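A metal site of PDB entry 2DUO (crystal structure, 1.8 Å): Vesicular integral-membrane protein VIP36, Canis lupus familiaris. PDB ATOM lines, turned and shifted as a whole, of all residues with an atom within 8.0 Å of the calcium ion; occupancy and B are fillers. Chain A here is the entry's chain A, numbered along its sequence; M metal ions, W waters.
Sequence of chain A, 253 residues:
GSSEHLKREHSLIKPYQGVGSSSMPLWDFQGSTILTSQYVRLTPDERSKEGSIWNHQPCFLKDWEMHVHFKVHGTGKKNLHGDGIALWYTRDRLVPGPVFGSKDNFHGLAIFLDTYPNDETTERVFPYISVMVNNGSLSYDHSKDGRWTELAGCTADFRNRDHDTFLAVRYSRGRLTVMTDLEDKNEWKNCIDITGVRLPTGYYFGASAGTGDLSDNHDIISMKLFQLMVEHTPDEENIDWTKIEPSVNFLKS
The side-chain amide nitrogen (ND2) of Asn 118 sits at hydrogen-bond distance from a ring nitrogen (NE2) of His 142 (3.4 Å).
OD1 of Asp 145 sits at hydrogen-bond distance from N of Asp 119 (2.9 Å).
The backbone carbonyl oxygen of Asp 145 lies within hydrogen-bond range of the guanidinium group of Arg 124 (3.1 Å).
The side-chain carboxylate of Asp 114 sits close to the side-chain hydroxyl of Tyr 140, 3.3 Å away.
O of Asp 114 is in hydrogen-bond range of N of Tyr 128.
OD1 of Asn 118 is bound to the calcium ion, at 2.3 Å.
The backbone carbonyl oxygen (O) of Tyr 116 is bound to the calcium ion (2.4 Å).
OD2 of Asp 145 is bound to the calcium ion (2.4 Å).
The calcium ion is bound by water W2 (2.4 Å).
OD2 of Asp 114 is bound to the calcium ion, 2.5 Å away.
Water W1 is bound to the calcium ion (2.5 Å).
OD1 of Asp 114 binds the calcium ion (2.6 Å).
Water W2 bridges the side-chain hydroxyl (OH) of Tyr 140 (2.8 Å) and a ring nitrogen (ND1) of His 142 (2.9 Å).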
ATOM      1  N   HIS A  81       8.727   0.488 -21.576  1.00  0.00           N
ATOM      2  CA  HIS A  81       9.609  -0.435 -20.856  1.00  0.00           C
ATOM      3  C   HIS A  81       8.831  -1.021 -19.702  1.00  0.00           C
ATOM      4  O   HIS A  81       7.781  -0.501 -19.321  1.00  0.00           O
ATOM      5  CB  HIS A  81      10.842   0.297 -20.304  1.00  0.00           C
ATOM      6  CG  HIS A  81      10.485   1.439 -19.417  1.00  0.00           C
ATOM      7  ND1 HIS A  81      10.524   2.749 -19.844  1.00  0.00           N
ATOM      8  CD2 HIS A  81      10.008   1.467 -18.149  1.00  0.00           C
ATOM      9  CE1 HIS A  81      10.114   3.536 -18.866  1.00  0.00           C
ATOM     10  NE2 HIS A  81       9.788   2.783 -17.832  1.00  0.00           N
ATOM     11  N   GLY A  82       9.329  -2.114 -19.144  1.00  0.00           N
ATOM     12  CA  GLY A  82       8.669  -2.787 -18.030  1.00  0.00           C
ATOM     13  C   GLY A  82       9.270  -4.145 -17.812  1.00  0.00           C
ATOM     14  O   GLY A  82      10.121  -4.585 -18.587  1.00  0.00           O
ATOM     15  N   ASP A  83       8.821  -4.851 -16.754  1.00  0.00           N
ATOM     16  CA  ASP A  83       7.769  -4.387 -15.826  1.00  0.00           C
ATOM     17  C   ASP A  83       8.375  -3.829 -14.528  1.00  0.00           C
ATOM     18  O   ASP A  83       7.803  -2.930 -13.880  1.00  0.00           O
ATOM     19  CB  ASP A  83       6.851  -5.569 -15.434  1.00  0.00           C
ATOM     20  CG  ASP A  83       6.148  -6.228 -16.651  1.00  0.00           C
ATOM     21  OD1 ASP A  83       5.948  -7.467 -16.634  1.00  0.00           O
ATOM     22  OD2 ASP A  83       5.772  -5.521 -17.603  1.00  0.00           O
ATOM     23  N   GLY A  84       9.528  -4.395 -14.149  1.00  0.00           N
ATOM     24  CA  GLY A  84      10.189  -3.996 -12.924  1.00  0.00           C
ATOM     25  C   GLY A  84      10.764  -5.183 -12.166  1.00  0.00           C
ATOM     26  O   GLY A  84      10.736  -6.316 -12.644  1.00  0.00           O
ATOM     27  N   PHE A 100       5.860  -9.216 -11.006  1.00  0.00           N
ATOM     28  CA  PHE A 100       7.263  -8.978 -11.416  1.00  0.00           C
ATOM     29  C   PHE A 100       8.004 -10.309 -11.522  1.00  0.00           C
ATOM     30  O   PHE A 100       9.102 -10.473 -10.958  1.00  0.00           O
ATOM     31  CB  PHE A 100       7.954  -7.996 -10.445  1.00  0.00           C
ATOM     32  CG  PHE A 100       7.249  -6.694 -10.338  1.00  0.00           C
ATOM     33  CD1 PHE A 100       7.356  -5.722 -11.350  1.00  0.00           C
ATOM     34  CD2 PHE A 100       6.382  -6.451  -9.290  1.00  0.00           C
ATOM     35  CE1 PHE A 100       6.665  -4.522 -11.281  1.00  0.00           C
ATOM     36  CE2 PHE A 100       5.705  -5.258  -9.202  1.00  0.00           C
ATOM     37  CZ  PHE A 100       5.824  -4.288 -10.209  1.00  0.00           C
ATOM     38  N   LEU A 113       9.924  -2.612  -7.321  1.00  0.00           N
ATOM     39  CA  LEU A 113      10.551  -1.554  -8.081  1.00  0.00           C
ATOM     40  C   LEU A 113       9.856  -1.529  -9.429  1.00  0.00           C
ATOM     41  O   LEU A 113      10.291  -2.219 -10.352  1.00  0.00           O
ATOM     42  CB  LEU A 113      12.040  -1.827  -8.247  1.00  0.00           C
ATOM     43  CG  LEU A 113      12.874  -1.677  -6.967  1.00  0.00           C
ATOM     44  CD1 LEU A 113      12.839  -2.923  -6.095  1.00  0.00           C
ATOM     45  CD2 LEU A 113      14.296  -1.439  -7.402  1.00  0.00           C
ATOM     46  N   ASP A 114       8.807  -0.709  -9.530  1.00  0.00           N
ATOM     47  CA  ASP A 114       7.832  -0.806 -10.627  1.00  0.00           C
ATOM     48  C   ASP A 114       8.165   0.307 -11.584  1.00  0.00           C
ATOM     49  O   ASP A 114       8.087   1.474 -11.205  1.00  0.00           O
ATOM     50  CB  ASP A 114       6.411  -0.617 -10.055  1.00  0.00           C
ATOM     51  CG  ASP A 114       5.321  -0.740 -11.130  1.00  0.00           C
ATOM     52  OD1 ASP A 114       4.137  -0.849 -10.754  1.00  0.00           O
ATOM     53  OD2 ASP A 114       5.647  -0.716 -12.331  1.00  0.00           O
ATOM     54  N   THR A 115       8.555  -0.049 -12.815  1.00  0.00           N
ATOM     55  CA  THR A 115       9.036   0.952 -13.748  1.00  0.00           C
ATOM     56  C   THR A 115       7.978   1.568 -14.655  1.00  0.00           C
ATOM     57  O   THR A 115       8.247   2.603 -15.276  1.00  0.00           O
ATOM     58  CB  THR A 115      10.180   0.422 -14.620  1.00  0.00           C
ATOM     59  OG1 THR A 115       9.670  -0.641 -15.426  1.00  0.00           O
ATOM     60  CG2 THR A 115      11.344  -0.072 -13.740  1.00  0.00           C
ATOM     61  N   TYR A 116       6.775   0.983 -14.714  1.00  0.00           N
ATOM     62  CA  TYR A 116       5.801   1.369 -15.742  1.00  0.00           C
ATOM     63  C   TYR A 116       4.384   1.596 -15.200  1.00  0.00           C
ATOM     64  O   TYR A 116       3.860   0.721 -14.549  1.00  0.00           O
ATOM     65  CB  TYR A 116       5.758   0.311 -16.858  1.00  0.00           C
ATOM     66  CG  TYR A 116       4.786   0.640 -17.974  1.00  0.00           C
ATOM     67  CD1 TYR A 116       5.135   1.538 -18.986  1.00  0.00           C
ATOM     68  CD2 TYR A 116       3.502   0.062 -17.991  1.00  0.00           C
ATOM     69  CE1 TYR A 116       4.234   1.861 -20.001  1.00  0.00           C
ATOM     70  CE2 TYR A 116       2.586   0.363 -19.031  1.00  0.00           C
ATOM     71  CZ  TYR A 116       2.972   1.272 -20.018  1.00  0.00           C
ATOM     72  OH  TYR A 116       2.089   1.576 -21.044  1.00  0.00           O
ATOM     73  N   PRO A 117       3.767   2.786 -15.497  1.00  0.00           N
ATOM     74  CA  PRO A 117       2.391   3.017 -15.027  1.00  0.00           C
ATOM     75  C   PRO A 117       1.381   2.230 -15.870  1.00  0.00           C
ATOM     76  O   PRO A 117       0.983   2.667 -16.959  1.00  0.00           O
ATOM     77  CB  PRO A 117       2.208   4.524 -15.196  1.00  0.00           C
ATOM     78  CG  PRO A 117       3.135   4.908 -16.350  1.00  0.00           C
ATOM     79  CD  PRO A 117       4.294   3.925 -16.275  1.00  0.00           C
ATOM     80  N   ASN A 118       0.988   1.077 -15.366  1.00  0.00           N
ATOM     81  CA  ASN A 118      -0.068   0.299 -16.008  1.00  0.00           C
ATOM     82  C   ASN A 118      -1.407   0.988 -15.838  1.00  0.00           C
ATOM     83  O   ASN A 118      -2.294   0.862 -16.678  1.00  0.00           O
ATOM     84  CB  ASN A 118      -0.134  -1.122 -15.432  1.00  0.00           C
ATOM     85  CG  ASN A 118       1.105  -1.930 -15.753  1.00  0.00           C
ATOM     86  OD1 ASN A 118       2.111  -1.861 -15.048  1.00  0.00           O
ATOM     87  ND2 ASN A 118       1.036  -2.704 -16.844  1.00  0.00           N
ATOM     88  N   ASP A 119      -1.523   1.725 -14.730  1.00  0.00           N
ATOM     89  CA  ASP A 119      -2.772   2.358 -14.329  1.00  0.00           C
ATOM     90  C   ASP A 119      -2.997   3.642 -15.123  1.00  0.00           C
ATOM     91  O   ASP A 119      -2.272   4.633 -14.932  1.00  0.00           O
ATOM     92  CB  ASP A 119      -2.741   2.619 -12.813  1.00  0.00           C
ATOM     93  CG  ASP A 119      -4.027   3.231 -12.257  1.00  0.00           C
ATOM     94  OD1 ASP A 119      -4.984   3.459 -13.007  1.00  0.00           O
ATOM     95  OD2 ASP A 119      -4.081   3.480 -11.032  1.00  0.00           O
ATOM     96  N   ARG A 124       0.412   8.584  -9.338  1.00  0.00           N
ATOM     97  CA  ARG A 124       1.809   8.427  -8.990  1.00  0.00           C
ATOM     98  C   ARG A 124       2.704   8.696 -10.221  1.00  0.00           C
ATOM     99  O   ARG A 124       2.235   8.606 -11.377  1.00  0.00           O
ATOM    100  CB  ARG A 124       2.053   7.031  -8.385  1.00  0.00           C
ATOM    101  CG  ARG A 124       1.380   6.830  -7.005  1.00  0.00           C
ATOM    102  CD  ARG A 124       1.447   5.369  -6.474  1.00  0.00           C
ATOM    103  NE  ARG A 124       0.475   4.493  -7.135  1.00  0.00           N
ATOM    104  CZ  ARG A 124       0.473   3.163  -7.043  1.00  0.00           C
ATOM    105  NH1 ARG A 124       1.392   2.547  -6.309  1.00  0.00           N
ATOM    106  NH2 ARG A 124      -0.440   2.432  -7.678  1.00  0.00           N
ATOM    107  N   PHE A 126       6.271   7.466 -12.046  1.00  0.00           N
ATOM    108  CA  PHE A 126       7.086   6.253 -12.147  1.00  0.00           C
ATOM    109  C   PHE A 126       8.514   6.533 -12.634  1.00  0.00           C
ATOM    110  O   PHE A 126       8.734   7.549 -13.305  1.00  0.00           O
ATOM    111  CB  PHE A 126       6.377   5.206 -13.044  1.00  0.00           C
ATOM    112  CG  PHE A 126       5.147   4.628 -12.402  1.00  0.00           C
ATOM    113  CD1 PHE A 126       3.992   5.388 -12.257  1.00  0.00           C
ATOM    114  CD2 PHE A 126       5.160   3.327 -11.898  1.00  0.00           C
ATOM    115  CE1 PHE A 126       2.875   4.868 -11.624  1.00  0.00           C
ATOM    116  CE2 PHE A 126       4.059   2.803 -11.267  1.00  0.00           C
ATOM    117  CZ  PHE A 126       2.921   3.559 -11.125  1.00  0.00           C
ATOM    118  N   TYR A 128       8.274   3.698  -9.445  1.00  0.00           N
ATOM    119  CA  TYR A 128       7.673   3.865  -8.130  1.00  0.00           C
ATOM    120  C   TYR A 128       8.032   2.648  -7.303  1.00  0.00           C
ATOM    121  O   TYR A 128       7.765   1.512  -7.707  1.00  0.00           O
ATOM    122  CB  TYR A 128       6.130   4.024  -8.262  1.00  0.00           C
ATOM    123  CG  TYR A 128       5.490   4.508  -6.969  1.00  0.00           C
ATOM    124  CD1 TYR A 128       5.466   5.884  -6.637  1.00  0.00           C
ATOM    125  CD2 TYR A 128       4.960   3.607  -6.058  1.00  0.00           C
ATOM    126  CE1 TYR A 128       4.889   6.320  -5.439  1.00  0.00           C
ATOM    127  CE2 TYR A 128       4.395   4.022  -4.839  1.00  0.00           C
ATOM    128  CZ  TYR A 128       4.352   5.368  -4.541  1.00  0.00           C
ATOM    129  OH  TYR A 128       3.763   5.745  -3.368  1.00  0.00           O
ATOM    130  N   TYR A 140      -1.803  -8.942  -5.950  1.00  0.00           N
ATOM    131  CA  TYR A 140      -1.221  -7.730  -6.508  1.00  0.00           C
ATOM    132  C   TYR A 140      -1.923  -7.429  -7.822  1.00  0.00           C
ATOM    133  O   TYR A 140      -1.855  -8.227  -8.758  1.00  0.00           O
ATOM    134  CB  TYR A 140       0.274  -7.945  -6.774  1.00  0.00           C
ATOM    135  CG  TYR A 140       0.938  -6.781  -7.452  1.00  0.00           C
ATOM    136  CD1 TYR A 140       1.293  -5.643  -6.731  1.00  0.00           C
ATOM    137  CD2 TYR A 140       1.219  -6.825  -8.825  1.00  0.00           C
ATOM    138  CE1 TYR A 140       1.925  -4.547  -7.374  1.00  0.00           C
ATOM    139  CE2 TYR A 140       1.838  -5.727  -9.474  1.00  0.00           C
ATOM    140  CZ  TYR A 140       2.168  -4.612  -8.737  1.00  0.00           C
ATOM    141  OH  TYR A 140       2.782  -3.542  -9.382  1.00  0.00           O
ATOM    142  N   ASP A 141      -2.589  -6.293  -7.906  1.00  0.00           N
ATOM    143  CA  ASP A 141      -3.293  -5.952  -9.140  1.00  0.00           C
ATOM    144  C   ASP A 141      -2.345  -5.216 -10.098  1.00  0.00           C
ATOM    145  O   ASP A 141      -2.189  -3.988 -10.054  1.00  0.00           O
ATOM    146  CB  ASP A 141      -4.526  -5.091  -8.852  1.00  0.00           C
ATOM    147  CG  ASP A 141      -5.338  -4.810 -10.087  1.00  0.00           C
ATOM    148  OD1 ASP A 141      -6.460  -4.308  -9.924  1.00  0.00           O
ATOM    149  OD2 ASP A 141      -4.879  -5.105 -11.213  1.00  0.00           O
ATOM    150  N   HIS A 142      -1.691  -6.002 -10.959  1.00  0.00           N
ATOM    151  CA  HIS A 142      -0.637  -5.501 -11.850  1.00  0.00           C
ATOM    152  C   HIS A 142      -1.174  -4.389 -12.775  1.00  0.00           C
ATOM    153  O   HIS A 142      -0.513  -3.352 -12.990  1.00  0.00           O
ATOM    154  CB  HIS A 142      -0.039  -6.666 -12.637  1.00  0.00           C
ATOM    155  CG  HIS A 142       0.941  -6.233 -13.690  1.00  0.00           C
ATOM    156  ND1 HIS A 142       2.234  -5.855 -13.388  1.00  0.00           N
ATOM    157  CD2 HIS A 142       0.811  -6.100 -15.027  1.00  0.00           C
ATOM    158  CE1 HIS A 142       2.864  -5.519 -14.505  1.00  0.00           C
ATOM    159  NE2 HIS A 142       2.024  -5.649 -15.513  1.00  0.00           N
ATOM    160  N   SER A 143      -2.392  -4.585 -13.275  1.00  0.00           N
ATOM    161  CA  SER A 143      -3.056  -3.599 -14.127  1.00  0.00           C
ATOM    162  C   SER A 143      -3.215  -2.217 -13.487  1.00  0.00           C
ATOM    163  O   SER A 143      -3.361  -1.220 -14.203  1.00  0.00           O
ATOM    164  CB  SER A 143      -4.398  -4.138 -14.648  1.00  0.00           C
ATOM    165  OG  SER A 143      -5.443  -4.000 -13.699  1.00  0.00           O
ATOM    166  N   LYS A 144      -3.172  -2.144 -12.146  1.00  0.00           N
ATOM    167  CA  LYS A 144      -3.340  -0.879 -11.416  1.00  0.00           C
ATOM    168  C   LYS A 144      -2.118  -0.563 -10.540  1.00  0.00           C
ATOM    169  O   LYS A 144      -2.213   0.194  -9.572  1.00  0.00           O
ATOM    170  CB  LYS A 144      -4.628  -0.893 -10.572  1.00  0.00           C
ATOM    171  CG  LYS A 144      -5.909  -1.098 -11.410  1.00  0.00           C
ATOM    172  CD  LYS A 144      -6.293   0.122 -12.249  1.00  0.00           C
ATOM    173  CE  LYS A 144      -6.813   1.267 -11.400  1.00  0.00           C
ATOM    174  NZ  LYS A 144      -7.300   2.399 -12.275  1.00  0.00           N
ATOM    175  N   ASP A 145      -0.978  -1.129 -10.925  1.00  0.00           N
ATOM    176  CA  ASP A 145       0.293  -0.955 -10.207  1.00  0.00           C
ATOM    177  C   ASP A 145       0.143  -1.199  -8.699  1.00  0.00           C
ATOM    178  O   ASP A 145       0.708  -0.450  -7.887  1.00  0.00           O
ATOM    179  CB  ASP A 145       0.834   0.461 -10.472  1.00  0.00           C
ATOM    180  CG  ASP A 145       0.808   0.820 -11.961  1.00  0.00           C
ATOM    181  OD1 ASP A 145       0.136   1.807 -12.325  1.00  0.00           O
ATOM    182  OD2 ASP A 145       1.463   0.089 -12.744  1.00  0.00           O
ATOM    183  N   GLY A 146      -0.654  -2.211  -8.337  1.00  0.00           N
ATOM    184  CA  GLY A 146      -0.871  -2.567  -6.934  1.00  0.00           C
ATOM    185  C   GLY A 146      -1.469  -1.482  -6.050  1.00  0.00           C
ATOM    186  O   GLY A 146      -1.281  -1.504  -4.825  1.00  0.00           O
HETATM  187 CA    CA M   1       3.415  -1.197 -13.234  1.00  0.00          CA
HETATM  188  O   HOH W   1       5.005  -2.581 -14.506  1.00  0.00           O
HETATM  189  O   HOH W   2       2.491  -3.202 -12.176  1.00  0.00           O
